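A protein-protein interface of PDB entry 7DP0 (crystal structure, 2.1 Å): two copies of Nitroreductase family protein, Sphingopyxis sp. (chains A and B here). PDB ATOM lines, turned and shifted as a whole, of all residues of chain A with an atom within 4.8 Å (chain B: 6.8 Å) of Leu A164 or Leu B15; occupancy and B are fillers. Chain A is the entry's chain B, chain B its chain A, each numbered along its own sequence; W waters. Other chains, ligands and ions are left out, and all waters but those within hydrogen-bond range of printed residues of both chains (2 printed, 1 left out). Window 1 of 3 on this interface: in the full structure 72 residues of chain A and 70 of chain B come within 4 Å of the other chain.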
ATOM      1  N   ILE A  37       1.042  -9.805  23.877  1.00  0.00           N
ATOM      2  CA  ILE A  37      -0.310  -9.285  23.894  1.00  0.00           C
ATOM      3  C   ILE A  37      -1.275 -10.302  23.282  1.00  0.00           C
ATOM      4  O   ILE A  37      -2.376 -10.538  23.794  1.00  0.00           O
ATOM      5  CB  ILE A  37      -0.385  -7.952  23.134  1.00  0.00           C
ATOM      6  CG1 ILE A  37       0.313  -6.855  23.938  1.00  0.00           C
ATOM      7  CG2 ILE A  37      -1.834  -7.588  22.829  1.00  0.00           C
ATOM      8  CD1 ILE A  37       0.785  -5.683  23.112  1.00  0.00           C
ATOM      9  N   ILE A  40      -2.030 -13.260  25.559  1.00  0.00           N
ATOM     10  CA  ILE A  40      -3.120 -12.962  26.476  1.00  0.00           C
ATOM     11  C   ILE A  40      -4.475 -12.855  25.773  1.00  0.00           C
ATOM     12  O   ILE A  40      -5.494 -13.329  26.288  1.00  0.00           O
ATOM     13  CB  ILE A  40      -2.876 -11.642  27.209  1.00  0.00           C
ATOM     14  CG1 ILE A  40      -1.515 -11.647  27.881  1.00  0.00           C
ATOM     15  CG2 ILE A  40      -3.992 -11.368  28.211  1.00  0.00           C
ATOM     16  CD1 ILE A  40      -1.098 -10.282  28.349  1.00  0.00           C
ATOM     17  N   ALA A  41      -4.487 -12.221  24.601  1.00  0.00           N
ATOM     18  CA  ALA A  41      -5.740 -11.982  23.882  1.00  0.00           C
ATOM     19  C   ALA A  41      -6.430 -13.293  23.480  1.00  0.00           C
ATOM     20  O   ALA A  41      -7.645 -13.334  23.259  1.00  0.00           O
ATOM     21  CB  ALA A  41      -5.494 -11.118  22.652  1.00  0.00           C
ATOM     22  N   ARG A  43      -7.003 -15.633  25.305  1.00  0.00           N
ATOM     23  CA  ARG A  43      -7.898 -16.005  26.414  1.00  0.00           C
ATOM     24  C   ARG A  43      -9.322 -15.480  26.236  1.00  0.00           C
ATOM     25  O   ARG A  43     -10.213 -15.747  27.057  1.00  0.00           O
ATOM     26  CB  ARG A  43      -7.346 -15.495  27.735  1.00  0.00           C
ATOM     27  CG  ARG A  43      -5.937 -16.000  28.071  1.00  0.00           C
ATOM     28  CD  ARG A  43      -5.839 -17.533  28.051  1.00  0.00           C
ATOM     29  NE  ARG A  43      -6.903 -18.185  28.810  1.00  0.00           N
ATOM     30  CZ  ARG A  43      -6.978 -19.500  29.024  1.00  0.00           C
ATOM     31  NH1 ARG A  43      -6.036 -20.316  28.563  1.00  0.00           N
ATOM     32  NH2 ARG A  43      -7.990 -20.010  29.710  1.00  0.00           N
ATOM     33  N   ALA A  44      -9.536 -14.733  25.161  1.00  0.00           N
ATOM     34  CA  ALA A  44     -10.878 -14.309  24.801  1.00  0.00           C
ATOM     35  C   ALA A  44     -11.794 -15.562  24.689  1.00  0.00           C
ATOM     36  O   ALA A  44     -11.338 -16.648  24.319  1.00  0.00           O
ATOM     37  CB  ALA A  44     -10.847 -13.528  23.510  1.00  0.00           C
ATOM     38  N   SER A 160     -10.354  -7.481  22.827  1.00  0.00           N
ATOM     39  CA  SER A 160      -9.310  -7.913  23.747  1.00  0.00           C
ATOM     40  C   SER A 160      -7.955  -7.357  23.307  1.00  0.00           C
ATOM     41  O   SER A 160      -7.202  -6.884  24.143  1.00  0.00           O
ATOM     42  CB  SER A 160      -9.223  -9.447  23.848  1.00  0.00           C
ATOM     43  OG  SER A 160     -10.428 -10.026  24.337  1.00  0.00           O
ATOM     44  N   VAL A 161      -7.643  -7.455  22.008  1.00  0.00           N
ATOM     45  CA  VAL A 161      -6.391  -6.928  21.481  1.00  0.00           C
ATOM     46  C   VAL A 161      -6.293  -5.409  21.688  1.00  0.00           C
ATOM     47  O   VAL A 161      -5.285  -4.909  22.175  1.00  0.00           O
ATOM     48  CB  VAL A 161      -6.202  -7.270  19.988  1.00  0.00           C
ATOM     49  CG1 VAL A 161      -4.905  -6.620  19.450  1.00  0.00           C
ATOM     50  CG2 VAL A 161      -6.141  -8.775  19.810  1.00  0.00           C
ATOM     51  N   MET A 162      -7.343  -4.682  21.314  1.00  0.00           N
ATOM     52  CA  MET A 162      -7.357  -3.227  21.438  1.00  0.00           C
ATOM     53  C   MET A 162      -7.197  -2.762  22.891  1.00  0.00           C
ATOM     54  O   MET A 162      -6.467  -1.816  23.137  1.00  0.00           O
ATOM     55  CB  MET A 162      -8.638  -2.645  20.820  1.00  0.00           C
ATOM     56  CG  MET A 162      -8.673  -2.879  19.334  1.00  0.00           C
ATOM     57  SD  MET A 162     -10.000  -2.045  18.476  1.00  0.00           S
ATOM     58  CE  MET A 162     -11.419  -3.147  18.695  1.00  0.00           C
ATOM     59  N   LEU A 163      -7.863  -3.413  23.844  1.00  0.00           N
ATOM     60  CA  LEU A 163      -7.674  -3.052  25.258  1.00  0.00           C
ATOM     61  C   LEU A 163      -6.249  -3.313  25.764  1.00  0.00           C
ATOM     62  O   LEU A 163      -5.697  -2.527  26.543  1.00  0.00           O
ATOM     63  CB  LEU A 163      -8.656  -3.803  26.145  1.00  0.00           C
ATOM     64  CG  LEU A 163     -10.125  -3.417  25.884  1.00  0.00           C
ATOM     65  CD1 LEU A 163     -11.062  -4.207  26.774  1.00  0.00           C
ATOM     66  CD2 LEU A 163     -10.354  -1.935  26.065  1.00  0.00           C
ATOM     67  N   LEU A 164      -5.664  -4.432  25.348  1.00  0.00           N
ATOM     68  CA  LEU A 164      -4.311  -4.780  25.798  1.00  0.00           C
ATOM     69  C   LEU A 164      -3.279  -3.812  25.232  1.00  0.00           C
ATOM     70  O   LEU A 164      -2.278  -3.498  25.885  1.00  0.00           O
ATOM     71  CB  LEU A 164      -3.965  -6.218  25.403  1.00  0.00           C
ATOM     72  CG  LEU A 164      -4.578  -7.339  26.256  1.00  0.00           C
ATOM     73  CD1 LEU A 164      -4.610  -8.652  25.506  1.00  0.00           C
ATOM     74  CD2 LEU A 164      -3.791  -7.525  27.547  1.00  0.00           C
ATOM     75  N   LEU A 165      -3.504  -3.354  24.006  1.00  0.00           N
ATOM     76  CA  LEU A 165      -2.577  -2.406  23.398  1.00  0.00           C
ATOM     77  C   LEU A 165      -2.535  -1.139  24.233  1.00  0.00           C
ATOM     78  O   LEU A 165      -1.457  -0.649  24.603  1.00  0.00           O
ATOM     79  CB  LEU A 165      -2.992  -2.087  21.968  1.00  0.00           C
ATOM     80  CG  LEU A 165      -2.637  -3.178  20.972  1.00  0.00           C
ATOM     81  CD1 LEU A 165      -3.384  -2.933  19.679  1.00  0.00           C
ATOM     82  CD2 LEU A 165      -1.124  -3.170  20.751  1.00  0.00           C
ATOM     83  N   VAL A 166      -3.728  -0.635  24.553  1.00  0.00           N
ATOM     84  CA  VAL A 166      -3.860   0.575  25.346  1.00  0.00           C
ATOM     85  C   VAL A 166      -3.179   0.396  26.716  1.00  0.00           C
ATOM     86  O   VAL A 166      -2.457   1.283  27.178  1.00  0.00           O
ATOM     87  CB  VAL A 166      -5.358   0.963  25.512  1.00  0.00           C
ATOM     88  CG1 VAL A 166      -5.541   2.057  26.549  1.00  0.00           C
ATOM     89  CG2 VAL A 166      -5.929   1.421  24.180  1.00  0.00           C
ATOM     90  N   GLU A 167      -3.380  -0.762  27.346  1.00  0.00           N
ATOM     91  CA  GLU A 167      -2.744  -1.038  28.632  1.00  0.00           C
ATOM     92  C   GLU A 167      -1.226  -0.926  28.548  1.00  0.00           C
ATOM     93  O   GLU A 167      -0.582  -0.502  29.512  1.00  0.00           O
ATOM     94  CB  GLU A 167      -3.119  -2.434  29.141  1.00  0.00           C
ATOM     95  CG  GLU A 167      -2.493  -2.795  30.493  1.00  0.00           C
ATOM     96  CD  GLU A 167      -2.786  -4.236  30.907  1.00  0.00           C
ATOM     97  OE1 GLU A 167      -2.266  -5.161  30.254  1.00  0.00           O
ATOM     98  OE2 GLU A 167      -3.548  -4.447  31.874  1.00  0.00           O
ATOM     99  N   HIS A 168      -0.668  -1.277  27.387  1.00  0.00           N
ATOM    100  CA  HIS A 168       0.786  -1.304  27.196  1.00  0.00           C
ATOM    101  C   HIS A 168       1.319  -0.042  26.554  1.00  0.00           C
ATOM    102  O   HIS A 168       2.426  -0.040  26.014  1.00  0.00           O
ATOM    103  CB  HIS A 168       1.212  -2.491  26.323  1.00  0.00           C
ATOM    104  CG  HIS A 168       1.068  -3.815  26.996  1.00  0.00           C
ATOM    105  ND1 HIS A 168      -0.132  -4.494  27.053  1.00  0.00           N
ATOM    106  CD2 HIS A 168       1.967  -4.576  27.665  1.00  0.00           C
ATOM    107  CE1 HIS A 168       0.039  -5.624  27.715  1.00  0.00           C
ATOM    108  NE2 HIS A 168       1.304  -5.695  28.099  1.00  0.00           N
ATOM    109  N   LEU B   9      -7.736  -4.173  39.530  1.00  0.00           N
ATOM    110  CA  LEU B   9      -7.509  -5.276  38.594  1.00  0.00           C
ATOM    111  C   LEU B   9      -7.208  -4.756  37.190  1.00  0.00           C
ATOM    112  O   LEU B   9      -8.040  -4.087  36.577  1.00  0.00           O
ATOM    113  CB  LEU B   9      -8.722  -6.213  38.564  1.00  0.00           C
ATOM    114  CG  LEU B   9      -8.488  -7.686  38.219  1.00  0.00           C
ATOM    115  CD1 LEU B   9      -7.517  -8.341  39.197  1.00  0.00           C
ATOM    116  CD2 LEU B   9      -9.813  -8.441  38.246  1.00  0.00           C
ATOM    117  N   SER B  10      -6.010  -5.064  36.694  1.00  0.00           N
ATOM    118  CA  SER B  10      -5.581  -4.618  35.366  1.00  0.00           C
ATOM    119  C   SER B  10      -6.349  -5.304  34.228  1.00  0.00           C
ATOM    120  O   SER B  10      -7.019  -6.314  34.437  1.00  0.00           O
ATOM    121  CB  SER B  10      -4.069  -4.838  35.205  1.00  0.00           C
ATOM    122  OG  SER B  10      -3.746  -6.129  34.720  1.00  0.00           O
ATOM    123  N   ALA B  11      -6.265  -4.738  33.027  1.00  0.00           N
ATOM    124  CA  ALA B  11      -6.908  -5.322  31.858  1.00  0.00           C
ATOM    125  C   ALA B  11      -6.384  -6.736  31.577  1.00  0.00           C
ATOM    126  O   ALA B  11      -7.151  -7.636  31.233  1.00  0.00           O
ATOM    127  CB  ALA B  11      -6.698  -4.440  30.639  1.00  0.00           C
ATOM    128  N   SER B  12      -5.074  -6.909  31.717  1.00  0.00           N
ATOM    129  CA  SER B  12      -4.430  -8.209  31.555  1.00  0.00           C
ATOM    130  C   SER B  12      -4.943  -9.220  32.573  1.00  0.00           C
ATOM    131  O   SER B  12      -5.265 -10.354  32.220  1.00  0.00           O
ATOM    132  CB  SER B  12      -2.909  -8.072  31.693  1.00  0.00           C
ATOM    133  OG  SER B  12      -2.317  -7.634  30.488  1.00  0.00           O
ATOM    134  N   GLU B  13      -4.995  -8.801  33.835  1.00  0.00           N
ATOM    135  CA  GLU B  13      -5.491  -9.633  34.931  1.00  0.00           C
ATOM    136  C   GLU B  13      -6.976  -9.973  34.748  1.00  0.00           C
ATOM    137  O   GLU B  13      -7.407 -11.087  35.034  1.00  0.00           O
ATOM    138  CB  GLU B  13      -5.296  -8.918  36.276  1.00  0.00           C
ATOM    139  CG  GLU B  13      -3.836  -8.693  36.651  1.00  0.00           C
ATOM    140  CD  GLU B  13      -3.627  -7.571  37.668  1.00  0.00           C
ATOM    141  OE1 GLU B  13      -4.571  -6.788  37.931  1.00  0.00           O
ATOM    142  OE2 GLU B  13      -2.493  -7.452  38.175  1.00  0.00           O
ATOM    143  N   ALA B  14      -7.762  -8.996  34.305  1.00  0.00           N
ATOM    144  CA  ALA B  14      -9.187  -9.221  34.092  1.00  0.00           C
ATOM    145  C   ALA B  14      -9.383 -10.272  33.008  1.00  0.00           C
ATOM    146  O   ALA B  14     -10.245 -11.146  33.134  1.00  0.00           O
ATOM    147  CB  ALA B  14      -9.907  -7.913  33.724  1.00  0.00           C
ATOM    148  N   LEU B  15      -8.579 -10.174  31.947  1.00  0.00           N
ATOM    149  CA  LEU B  15      -8.643 -11.103  30.810  1.00  0.00           C
ATOM    150  C   LEU B  15      -8.251 -12.536  31.195  1.00  0.00           C
ATOM    151  O   LEU B  15      -8.853 -13.516  30.743  1.00  0.00           O
ATOM    152  CB  LEU B  15      -7.723 -10.607  29.693  1.00  0.00           C
ATOM    153  CG  LEU B  15      -8.391  -9.951  28.481  1.00  0.00           C
ATOM    154  CD1 LEU B  15      -7.366  -9.119  27.746  1.00  0.00           C
ATOM    155  CD2 LEU B  15      -9.000 -10.982  27.548  1.00  0.00           C
ATOM    156  N   ALA B  16      -7.225 -12.642  32.032  1.00  0.00           N
ATOM    157  CA  ALA B  16      -6.717 -13.921  32.514  1.00  0.00           C
ATOM    158  C   ALA B  16      -7.724 -14.581  33.435  1.00  0.00           C
ATOM    159  O   ALA B  16      -7.919 -15.794  33.418  1.00  0.00           O
ATOM    160  CB  ALA B  16      -5.378 -13.709  33.259  1.00  0.00           C
ATOM    161  N   ARG B  17      -8.354 -13.760  34.263  1.00  0.00           N
ATOM    162  CA  ARG B  17      -9.245 -14.265  35.290  1.00  0.00           C
ATOM    163  C   ARG B  17     -10.647 -14.504  34.743  1.00  0.00           C
ATOM    164  O   ARG B  17     -11.453 -15.174  35.387  1.00  0.00           O
ATOM    165  CB  ARG B  17      -9.288 -13.296  36.483  1.00  0.00           C
ATOM    166  CG  ARG B  17      -8.026 -13.319  37.383  1.00  0.00           C
ATOM    167  CD  ARG B  17      -8.358 -12.657  38.733  1.00  0.00           C
ATOM    168  NE  ARG B  17      -7.282 -12.629  39.733  1.00  0.00           N
ATOM    169  CZ  ARG B  17      -6.048 -12.170  39.544  1.00  0.00           C
ATOM    170  NH1 ARG B  17      -5.686 -11.640  38.381  1.00  0.00           N
ATOM    171  NH2 ARG B  17      -5.174 -12.209  40.545  1.00  0.00           N
ATOM    172  N   ARG B  18     -10.947 -13.990  33.552  1.00  0.00           N
ATOM    173  CA  ARG B  18     -12.285 -14.225  33.004  1.00  0.00           C
ATOM    174  C   ARG B  18     -12.380 -15.644  32.475  1.00  0.00           C
ATOM    175  O   ARG B  18     -11.558 -16.067  31.668  1.00  0.00           O
ATOM    176  CB  ARG B  18     -12.652 -13.236  31.886  1.00  0.00           C
ATOM    177  CG  ARG B  18     -14.115 -13.380  31.421  1.00  0.00           C
ATOM    178  CD  ARG B  18     -14.294 -13.341  29.885  1.00  0.00           C
ATOM    179  NE  ARG B  18     -13.422 -14.317  29.233  1.00  0.00           N
ATOM    180  CZ  ARG B  18     -13.691 -15.613  29.072  1.00  0.00           C
ATOM    181  NH1 ARG B  18     -14.844 -16.142  29.492  1.00  0.00           N
ATOM    182  NH2 ARG B  18     -12.791 -16.390  28.473  1.00  0.00           N
ATOM    183  N   ARG B  19     -13.392 -16.368  32.946  1.00  0.00           N
ATOM    184  CA  ARG B  19     -13.712 -17.695  32.427  1.00  0.00           C
ATOM    185  C   ARG B  19     -15.213 -17.830  32.363  1.00  0.00           C
ATOM    186  O   ARG B  19     -15.936 -17.033  32.976  1.00  0.00           O
ATOM    187  CB  ARG B  19     -13.120 -18.797  33.319  1.00  0.00           C
ATOM    188  CG  ARG B  19     -13.884 -19.040  34.603  1.00  0.00           C
ATOM    189  CD  ARG B  19     -13.267 -20.204  35.414  1.00  0.00           C
ATOM    190  NE  ARG B  19     -13.450 -21.490  34.738  1.00  0.00           N
ATOM    191  CZ  ARG B  19     -12.550 -22.476  34.718  1.00  0.00           C
ATOM    192  NH1 ARG B  19     -11.397 -22.350  35.360  1.00  0.00           N
ATOM    193  NH2 ARG B  19     -12.810 -23.605  34.068  1.00  0.00           N
ATOM    194  N   GLN B 159     -17.621  -8.848  25.236  1.00  0.00           N
ATOM    195  CA  GLN B 159     -16.353  -9.107  25.919  1.00  0.00           C
ATOM    196  C   GLN B 159     -16.053  -7.968  26.898  1.00  0.00           C
ATOM    197  O   GLN B 159     -15.544  -8.209  27.987  1.00  0.00           O
ATOM    198  CB  GLN B 159     -15.203  -9.299  24.919  1.00  0.00           C
ATOM    199  CG  GLN B 159     -13.766  -9.382  25.531  1.00  0.00           C
ATOM    200  CD  GLN B 159     -13.509 -10.645  26.331  1.00  0.00           C
ATOM    201  OE1 GLN B 159     -14.433 -11.353  26.738  1.00  0.00           O
ATOM    202  NE2 GLN B 159     -12.239 -10.929  26.570  1.00  0.00           N
ATOM    203  N   LEU B 163     -15.354  -8.723  30.836  1.00  0.00           N
ATOM    204  CA  LEU B 163     -14.129  -8.249  31.494  1.00  0.00           C
ATOM    205  C   LEU B 163     -14.428  -7.308  32.661  1.00  0.00           C
ATOM    206  O   LEU B 163     -13.793  -7.399  33.714  1.00  0.00           O
ATOM    207  CB  LEU B 163     -13.222  -7.542  30.475  1.00  0.00           C
ATOM    208  CG  LEU B 163     -12.631  -8.489  29.413  1.00  0.00           C
ATOM    209  CD1 LEU B 163     -11.762  -7.762  28.386  1.00  0.00           C
ATOM    210  CD2 LEU B 163     -11.816  -9.594  30.092  1.00  0.00           C
ATOM    211  N   VAL B 166     -15.692  -9.181  35.874  1.00  0.00           N
ATOM    212  CA  VAL B 166     -14.544  -9.756  36.606  1.00  0.00           C
ATOM    213  C   VAL B 166     -13.756  -8.726  37.434  1.00  0.00           C
ATOM    214  O   VAL B 166     -13.355  -8.977  38.584  1.00  0.00           O
ATOM    215  CB  VAL B 166     -13.576 -10.452  35.612  1.00  0.00           C
ATOM    216  CG1 VAL B 166     -12.201 -10.704  36.256  1.00  0.00           C
ATOM    217  CG2 VAL B 166     -14.209 -11.745  35.089  1.00  0.00           C
HETATM  218  O   HOH W   1     -10.550 -18.783  30.781  1.00  0.00           O
HETATM  219  O   HOH W   2     -10.719 -13.494  28.571  1.00  0.00           O
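OE2 of Glu A167 lies within hydrogen-bond range of OG of Ser B10, at 3.3 Å.
N of Ala B11 sits at hydrogen-bond distance from OE2 of Glu A167 (3.0 Å).
OG of Ser B12 is in hydrogen-bond range of OE1 of Glu A167, 2.5 Å away.
The guanidinium group (NH2) of Arg B18 sits at hydrogen-bond distance from the backbone carbonyl oxygen (O) of Arg A43 (3.0 Å).
The side-chain hydroxyl (OG) of Ser A160 sits at hydrogen-bond distance from the side-chain amide nitrogen (NE2) of Gln B159 (3.0 Å).
The backbone NH (N) of Ser B12 lies close to the side-chain hydroxyl (OG) of Ser B10.
N of Ser B10 is in hydrogen-bond range of OE1 of Glu B13 (2.6 Å).
A ring nitrogen (ND1) of His A168 lies within hydrogen-bond range of the backbone carbonyl oxygen (O) of Leu A164, 2.6 Å away.
Among the printed residues, pairs that only touch across the chains: Leu A164 with Ser B12, Leu A164 with Leu B15, Ile A40 with Ser B12, Ser A160 with Leu B15, Arg A43 with Leu B15, Leu A163 with Leu B163 and Ala A44 with Arg B18.
Of the printed residues of chain B, Leu A164 touches Ser B12 (3.3 Å) and Leu B15 (3.6 Å).
Leu B15 touches just these residues of chain A: Arg A43 (3.9 Å), Ser A160 (3.6 Å) and Leu A164 (3.6 Å).
Printed residues of chain B within 4 Å of Ala A44: Arg B18.
Printed residues of chain B within 4 Å of Ile A40: Ser B12 (3.6 Å).
Of the printed residues of chain A, Leu B163 touches Leu A163.
Of the printed residues of chain B, Ser A160 touches Leu B15 (3.6 Å) and Gln B159 (3.0 Å).
The nearest residue of chain A that does not touch Leu B15 is Ile A40 (4.1 Å).
Of the 14 printed residues of chain B, 7 touch a printed residue of chain A.
Printed residues of chain A that touch a printed residue of chain B: Ile A40, Arg A43, Ala A44, Ser A160, Leu A163, Leu A164 and Glu A167.
Along chain A the printed residues that touch a printed residue of chain B span positions 40 to 167.
Leu B163 touches its own counterpart, Leu A163.
Positions printed for both chains: 163 and 166.
Of the 12 pairs that touch across the chains among the printed residues, 1 has its exchanged pair printed and touching as well.
Water W2 lies within hydrogen-bond range of the backbone carbonyl oxygen (O) of Arg A43 (2.8 Å), the backbone carbonyl oxygen (O) of Leu B15 (2.9 Å) and the guanidinium group (NE) of Arg B18 (2.9 Å).
Water W1 lies within hydrogen-bond range of the backbone carbonyl oxygen (O) of Arg B18 and the guanidinium group (NH2) of Arg A43.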
